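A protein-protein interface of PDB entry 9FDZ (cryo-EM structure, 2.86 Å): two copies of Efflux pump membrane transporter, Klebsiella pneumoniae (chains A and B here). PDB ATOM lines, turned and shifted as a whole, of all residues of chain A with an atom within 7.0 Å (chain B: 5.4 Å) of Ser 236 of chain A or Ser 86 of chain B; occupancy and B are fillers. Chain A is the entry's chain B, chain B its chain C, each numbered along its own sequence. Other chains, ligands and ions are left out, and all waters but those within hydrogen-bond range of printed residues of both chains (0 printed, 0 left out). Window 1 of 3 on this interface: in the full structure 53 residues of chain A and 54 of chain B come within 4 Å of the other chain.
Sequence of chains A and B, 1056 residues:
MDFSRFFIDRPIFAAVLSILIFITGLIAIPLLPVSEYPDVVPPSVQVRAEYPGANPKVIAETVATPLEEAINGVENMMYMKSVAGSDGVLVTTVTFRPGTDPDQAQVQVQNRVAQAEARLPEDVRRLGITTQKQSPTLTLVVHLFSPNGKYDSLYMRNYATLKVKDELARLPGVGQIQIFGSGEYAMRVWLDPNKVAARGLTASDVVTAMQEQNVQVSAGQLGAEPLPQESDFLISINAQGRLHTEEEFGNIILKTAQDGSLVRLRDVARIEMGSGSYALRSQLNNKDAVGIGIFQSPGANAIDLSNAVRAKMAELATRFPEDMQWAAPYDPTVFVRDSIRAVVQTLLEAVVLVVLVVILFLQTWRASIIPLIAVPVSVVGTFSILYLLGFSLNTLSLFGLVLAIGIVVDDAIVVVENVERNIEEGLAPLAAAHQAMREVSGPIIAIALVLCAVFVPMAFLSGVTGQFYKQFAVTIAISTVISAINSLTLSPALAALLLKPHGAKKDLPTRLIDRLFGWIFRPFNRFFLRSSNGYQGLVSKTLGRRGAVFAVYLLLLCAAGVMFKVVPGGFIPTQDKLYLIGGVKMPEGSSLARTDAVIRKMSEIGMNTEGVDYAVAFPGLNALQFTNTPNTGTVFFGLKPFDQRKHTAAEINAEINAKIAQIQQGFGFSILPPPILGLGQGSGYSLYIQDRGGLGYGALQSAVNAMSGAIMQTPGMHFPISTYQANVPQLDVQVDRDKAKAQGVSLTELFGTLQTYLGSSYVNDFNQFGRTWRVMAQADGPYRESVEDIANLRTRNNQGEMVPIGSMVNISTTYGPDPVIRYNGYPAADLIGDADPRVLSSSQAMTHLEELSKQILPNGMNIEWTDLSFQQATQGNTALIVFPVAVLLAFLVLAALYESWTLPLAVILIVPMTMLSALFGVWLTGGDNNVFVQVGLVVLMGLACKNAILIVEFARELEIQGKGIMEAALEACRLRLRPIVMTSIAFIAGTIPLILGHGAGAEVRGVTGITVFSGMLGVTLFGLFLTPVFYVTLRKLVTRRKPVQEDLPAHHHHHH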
ATOM      1  N   ALA A 219      23.021  -0.084 -17.357  1.00  0.00           N
ATOM      2  CA  ALA A 219      22.381  -0.767 -18.474  1.00  0.00           C
ATOM      3  C   ALA A 219      22.472  -0.002 -19.788  1.00  0.00           C
ATOM      4  O   ALA A 219      21.884  -0.439 -20.783  1.00  0.00           O
ATOM      5  CB  ALA A 219      20.916  -1.059 -18.142  1.00  0.00           C
ATOM      6  N   GLY A 220      23.187   1.120 -19.827  1.00  0.00           N
ATOM      7  CA  GLY A 220      23.375   1.817 -21.088  1.00  0.00           C
ATOM      8  C   GLY A 220      22.076   2.360 -21.649  1.00  0.00           C
ATOM      9  O   GLY A 220      21.191   2.812 -20.915  1.00  0.00           O
ATOM     10  N   GLN A 221      21.955   2.315 -22.977  1.00  0.00           N
ATOM     11  CA  GLN A 221      20.804   2.863 -23.680  1.00  0.00           C
ATOM     12  C   GLN A 221      20.323   1.874 -24.733  1.00  0.00           C
ATOM     13  O   GLN A 221      20.965   0.856 -25.004  1.00  0.00           O
ATOM     14  CB  GLN A 221      21.132   4.202 -24.350  1.00  0.00           C
ATOM     15  CG  GLN A 221      21.695   5.257 -23.425  1.00  0.00           C
ATOM     16  CD  GLN A 221      22.702   6.145 -24.120  1.00  0.00           C
ATOM     17  OE1 GLN A 221      22.461   7.333 -24.328  1.00  0.00           O
ATOM     18  NE2 GLN A 221      23.841   5.573 -24.486  1.00  0.00           N
ATOM     19  N   LEU A 222      19.179   2.192 -25.328  1.00  0.00           N
ATOM     20  CA  LEU A 222      18.631   1.453 -26.455  1.00  0.00           C
ATOM     21  C   LEU A 222      18.870   2.221 -27.750  1.00  0.00           C
ATOM     22  O   LEU A 222      18.918   3.452 -27.770  1.00  0.00           O
ATOM     23  CB  LEU A 222      17.132   1.205 -26.273  1.00  0.00           C
ATOM     24  CG  LEU A 222      16.697   0.167 -25.241  1.00  0.00           C
ATOM     25  CD1 LEU A 222      15.191   0.009 -25.276  1.00  0.00           C
ATOM     26  CD2 LEU A 222      17.378  -1.163 -25.497  1.00  0.00           C
ATOM     27  N   LEU A 234      16.523   7.352 -29.004  1.00  0.00           N
ATOM     28  CA  LEU A 234      17.588   6.875 -28.130  1.00  0.00           C
ATOM     29  C   LEU A 234      17.139   7.083 -26.694  1.00  0.00           C
ATOM     30  O   LEU A 234      16.983   8.226 -26.255  1.00  0.00           O
ATOM     31  CB  LEU A 234      18.901   7.609 -28.410  1.00  0.00           C
ATOM     32  CG  LEU A 234      20.081   7.361 -27.471  1.00  0.00           C
ATOM     33  CD1 LEU A 234      21.357   7.191 -28.270  1.00  0.00           C
ATOM     34  CD2 LEU A 234      20.228   8.508 -26.487  1.00  0.00           C
ATOM     35  N   ILE A 235      16.928   5.989 -25.969  1.00  0.00           N
ATOM     36  CA  ILE A 235      16.367   6.030 -24.625  1.00  0.00           C
ATOM     37  C   ILE A 235      17.304   5.303 -23.671  1.00  0.00           C
ATOM     38  O   ILE A 235      17.804   4.216 -23.983  1.00  0.00           O
ATOM     39  CB  ILE A 235      14.948   5.421 -24.589  1.00  0.00           C
ATOM     40  CG1 ILE A 235      14.387   5.433 -23.168  1.00  0.00           C
ATOM     41  CG2 ILE A 235      14.942   4.016 -25.169  1.00  0.00           C
ATOM     42  CD1 ILE A 235      12.893   5.220 -23.109  1.00  0.00           C
ATOM     43  N   SER A 236      17.556   5.914 -22.518  1.00  0.00           N
ATOM     44  CA  SER A 236      18.422   5.318 -21.513  1.00  0.00           C
ATOM     45  C   SER A 236      17.667   4.273 -20.703  1.00  0.00           C
ATOM     46  O   SER A 236      16.440   4.318 -20.577  1.00  0.00           O
ATOM     47  CB  SER A 236      18.984   6.390 -20.582  1.00  0.00           C
ATOM     48  OG  SER A 236      19.750   7.338 -21.301  1.00  0.00           O
ATOM     49  N   ILE A 237      18.417   3.327 -20.144  1.00  0.00           N
ATOM     50  CA  ILE A 237      17.866   2.243 -19.340  1.00  0.00           C
ATOM     51  C   ILE A 237      18.357   2.411 -17.911  1.00  0.00           C
ATOM     52  O   ILE A 237      19.563   2.552 -17.674  1.00  0.00           O
ATOM     53  CB  ILE A 237      18.264   0.866 -19.895  1.00  0.00           C
ATOM     54  CG1 ILE A 237      18.021   0.802 -21.401  1.00  0.00           C
ATOM     55  CG2 ILE A 237      17.491  -0.230 -19.191  1.00  0.00           C
ATOM     56  CD1 ILE A 237      18.549  -0.457 -22.042  1.00  0.00           C
ATOM     57  N   ASN A 238      17.428   2.397 -16.962  1.00  0.00           N
ATOM     58  CA  ASN A 238      17.733   2.572 -15.545  1.00  0.00           C
ATOM     59  C   ASN A 238      17.509   1.235 -14.844  1.00  0.00           C
ATOM     60  O   ASN A 238      16.417   0.951 -14.349  1.00  0.00           O
ATOM     61  CB  ASN A 238      16.873   3.672 -14.930  1.00  0.00           C
ATOM     62  CG  ASN A 238      17.052   5.005 -15.623  1.00  0.00           C
ATOM     63  OD1 ASN A 238      18.111   5.290 -16.180  1.00  0.00           O
ATOM     64  ND2 ASN A 238      16.013   5.831 -15.595  1.00  0.00           N
ATOM     65  N   ALA B  54      26.088   4.322 -17.199  1.00  0.00           N
ATOM     66  CA  ALA B  54      25.329   4.870 -16.085  1.00  0.00           C
ATOM     67  C   ALA B  54      24.490   6.058 -16.532  1.00  0.00           C
ATOM     68  O   ALA B  54      24.942   6.900 -17.312  1.00  0.00           O
ATOM     69  CB  ALA B  54      26.268   5.287 -14.955  1.00  0.00           C
ATOM     70  N   ASN B  55      23.261   6.120 -16.033  1.00  0.00           N
ATOM     71  CA  ASN B  55      22.372   7.230 -16.323  1.00  0.00           C
ATOM     72  C   ASN B  55      22.843   8.490 -15.604  1.00  0.00           C
ATOM     73  O   ASN B  55      23.566   8.412 -14.608  1.00  0.00           O
ATOM     74  CB  ASN B  55      20.945   6.874 -15.918  1.00  0.00           C
ATOM     75  CG  ASN B  55      20.769   6.777 -14.419  1.00  0.00           C
ATOM     76  OD1 ASN B  55      20.643   7.787 -13.728  1.00  0.00           O
ATOM     77  ND2 ASN B  55      20.754   5.554 -13.908  1.00  0.00           N
ATOM     78  N   PRO B  56      22.457   9.671 -16.101  1.00  0.00           N
ATOM     79  CA  PRO B  56      22.970  10.916 -15.501  1.00  0.00           C
ATOM     80  C   PRO B  56      22.676  11.063 -14.019  1.00  0.00           C
ATOM     81  O   PRO B  56      23.509  11.605 -13.284  1.00  0.00           O
ATOM     82  CB  PRO B  56      22.272  12.005 -16.323  1.00  0.00           C
ATOM     83  CG  PRO B  56      21.978  11.361 -17.623  1.00  0.00           C
ATOM     84  CD  PRO B  56      21.657   9.935 -17.309  1.00  0.00           C
ATOM     85  N   ALA B  84      26.728  15.985 -15.712  1.00  0.00           N
ATOM     86  CA  ALA B  84      26.735  14.544 -15.920  1.00  0.00           C
ATOM     87  C   ALA B  84      25.807  14.198 -17.074  1.00  0.00           C
ATOM     88  O   ALA B  84      24.624  14.552 -17.052  1.00  0.00           O
ATOM     89  CB  ALA B  84      26.302  13.806 -14.652  1.00  0.00           C
ATOM     90  N   GLY B  85      26.340  13.499 -18.072  1.00  0.00           N
ATOM     91  CA  GLY B  85      25.573  13.189 -19.262  1.00  0.00           C
ATOM     92  C   GLY B  85      25.192  11.730 -19.390  1.00  0.00           C
ATOM     93  O   GLY B  85      25.716  10.878 -18.669  1.00  0.00           O
ATOM     94  N   SER B  86      24.276  11.432 -20.315  1.00  0.00           N
ATOM     95  CA  SER B  86      23.833  10.058 -20.515  1.00  0.00           C
ATOM     96  C   SER B  86      24.917   9.183 -21.124  1.00  0.00           C
ATOM     97  O   SER B  86      24.809   7.953 -21.071  1.00  0.00           O
ATOM     98  CB  SER B  86      22.589  10.031 -21.401  1.00  0.00           C
ATOM     99  OG  SER B  86      22.795  10.781 -22.585  1.00  0.00           O
ATOM    100  N   ASP B  87      25.958   9.784 -21.702  1.00  0.00           N
ATOM    101  CA  ASP B  87      27.053   9.015 -22.277  1.00  0.00           C
ATOM    102  C   ASP B  87      27.921   8.344 -21.222  1.00  0.00           C
ATOM    103  O   ASP B  87      28.775   7.527 -21.580  1.00  0.00           O
ATOM    104  CB  ASP B  87      27.916   9.917 -23.159  1.00  0.00           C
ATOM    105  CG  ASP B  87      28.384  11.161 -22.435  1.00  0.00           C
ATOM    106  OD1 ASP B  87      27.778  11.511 -21.403  1.00  0.00           O
ATOM    107  OD2 ASP B  87      29.357  11.789 -22.898  1.00  0.00           O
ATOM    108  N   GLY B  88      27.729   8.662 -19.949  1.00  0.00           N
ATOM    109  CA  GLY B  88      28.517   8.082 -18.889  1.00  0.00           C
ATOM    110  C   GLY B  88      29.737   8.870 -18.476  1.00  0.00           C
ATOM    111  O   GLY B  88      30.603   8.313 -17.792  1.00  0.00           O
ATOM    112  N   PRO B 630      22.752  13.983 -27.174  1.00  0.00           N
ATOM    113  CA  PRO B 630      22.188  13.551 -28.466  1.00  0.00           C
ATOM    114  C   PRO B 630      21.285  14.576 -29.131  1.00  0.00           C
ATOM    115  O   PRO B 630      21.300  14.694 -30.363  1.00  0.00           O
ATOM    116  CB  PRO B 630      21.415  12.279 -28.092  1.00  0.00           C
ATOM    117  CG  PRO B 630      22.057  11.798 -26.839  1.00  0.00           C
ATOM    118  CD  PRO B 630      22.452  13.033 -26.092  1.00  0.00           C
ATOM    119  N   PRO B 729      12.689  10.939 -21.750  1.00  0.00           N
ATOM    120  CA  PRO B 729      12.174   9.584 -21.515  1.00  0.00           C
ATOM    121  C   PRO B 729      13.290   8.609 -21.173  1.00  0.00           C
ATOM    122  O   PRO B 729      14.384   8.656 -21.738  1.00  0.00           O
ATOM    123  CB  PRO B 729      11.503   9.221 -22.845  1.00  0.00           C
ATOM    124  CG  PRO B 729      11.311  10.519 -23.559  1.00  0.00           C
ATOM    125  CD  PRO B 729      12.427  11.402 -23.120  1.00  0.00           C
ATOM    126  N   GLN B 730      12.994   7.710 -20.236  1.00  0.00           N
ATOM    127  CA  GLN B 730      13.946   6.700 -19.796  1.00  0.00           C
ATOM    128  C   GLN B 730      13.194   5.409 -19.517  1.00  0.00           C
ATOM    129  O   GLN B 730      11.980   5.410 -19.298  1.00  0.00           O
ATOM    130  CB  GLN B 730      14.713   7.144 -18.545  1.00  0.00           C
ATOM    131  CG  GLN B 730      15.495   8.436 -18.705  1.00  0.00           C
ATOM    132  CD  GLN B 730      16.257   8.810 -17.454  1.00  0.00           C
ATOM    133  OE1 GLN B 730      16.058   8.219 -16.393  1.00  0.00           O
ATOM    134  NE2 GLN B 730      17.137   9.797 -17.571  1.00  0.00           N
ATOM    135  N   LEU B 731      13.930   4.303 -19.526  1.00  0.00           N
ATOM    136  CA  LEU B 731      13.375   2.994 -19.213  1.00  0.00           C
ATOM    137  C   LEU B 731      13.809   2.560 -17.822  1.00  0.00           C
ATOM    138  O   LEU B 731      14.988   2.653 -17.470  1.00  0.00           O
ATOM    139  CB  LEU B 731      13.812   1.947 -20.238  1.00  0.00           C
ATOM    140  CG  LEU B 731      12.999   1.865 -21.529  1.00  0.00           C
ATOM    141  CD1 LEU B 731      13.297   0.567 -22.247  1.00  0.00           C
ATOM    142  CD2 LEU B 731      11.516   1.985 -21.235  1.00  0.00           C
ATOM    143  N   ASP B 818      18.386  15.053 -18.136  1.00  0.00           N
ATOM    144  CA  ASP B 818      19.580  14.695 -18.891  1.00  0.00           C
ATOM    145  C   ASP B 818      20.011  15.877 -19.749  1.00  0.00           C
ATOM    146  O   ASP B 818      19.298  16.249 -20.689  1.00  0.00           O
ATOM    147  CB  ASP B 818      19.315  13.463 -19.758  1.00  0.00           C
ATOM    148  CG  ASP B 818      20.505  13.084 -20.621  1.00  0.00           C
ATOM    149  OD1 ASP B 818      21.641  13.484 -20.294  1.00  0.00           O
ATOM    150  OD2 ASP B 818      20.302  12.382 -21.633  1.00  0.00           O
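Printed residues of chain A that touch a printed residue of chain B: Gln 221, Leu 222, Leu 234, Ile 235, Ser 236, Ile 237 and Asn 238.
Among the printed residues, 13 pairs touch across the chains.
Among the printed residues, no Asp or Glu carboxylate lies within 4 Å of a Lys or Arg side-chain nitrogen of the other chain.
The backbone carbonyl oxygen of Gly 220 of chain A is in hydrogen-bond range of the backbone NH of Ile 237 of chain A, at 2.9 Å.
O of Ile 235 of chain A sits at hydrogen-bond distance from N of Leu 222 of chain A (2.8 Å).
The side-chain hydroxyl (OG) of Ser 86 of chain B lies within hydrogen-bond range of the side-chain carboxylate (OD2) of Asp 818 of chain B (3.1 Å).
No position is printed for both chains.
Of the 13 pairs that touch across the chains among the printed residues, none has its exchanged pair printed and touching as well.
The backbone NH of Leu 731 of chain B is in hydrogen-bond range of the backbone carbonyl oxygen of Ser 236 of chain A (2.7 Å).
OD1 of Asn 238 of chain A lies close to ND2 of Asn 55 of chain B.
OE1 of Gln 730 of chain B lies within hydrogen-bond range of ND2 of Asn 238 of chain A (2.5 Å).
The backbone carbonyl oxygen (O) of Leu 731 of chain B lies within hydrogen-bond range of the backbone NH (N) of Asn 238 of chain A.
Gln 221 of chain A touches Ser 86 of chain B.
Leu 731 of chain B touches Leu 222 of chain A (CD1 to CD1, 3.6 Å).
CD2 of Leu 234 of chain A touches CG of Pro 630 of chain B (3.8 Å).
Ile 235 of chain A touches Pro 729 of chain B (CG1 to O, 3.5 Å).
C of Gln 730 of chain B touches CD1 of Ile 235 of chain A, 3.6 Å away.
Ile 235 of chain A touches Leu 731 of chain B.
CB of Ser 86 of chain B touches OG of Ser 236 of chain A (3.9 Å).
Ser 236 of chain A touches Gln 730 of chain B.
Ile 237 of chain A touches Leu 731 of chain B (C to O, 3.4 Å).
Printed residues of chain B within 4 Å of Ser 236 of chain A: Ser 86, Gln 730 and Leu 731.
Of chain A, only Gln 221 (3.9 Å) and Ser 236 (3.9 Å) come within 4 Å of Ser 86 of chain B.
Gly 88 of chain B touches none of the printed residues of chain A.
Printed residues of chain A within 4 Å of Gln 730 of chain B: Ile 235 (3.6 Å), Ser 236 (3.5 Å) and Asn 238 (2.5 Å).
Of the printed residues of chain A, Leu 731 of chain B touches Leu 222 (3.6 Å), Ile 235 (3.7 Å), Ser 236 (2.7 Å), Ile 237 (3.4 Å) and Asn 238 (2.5 Å).
The nearest printed residue of chain A that does not touch Pro 729 of chain B is Ser 236 of chain A (4.3 Å).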
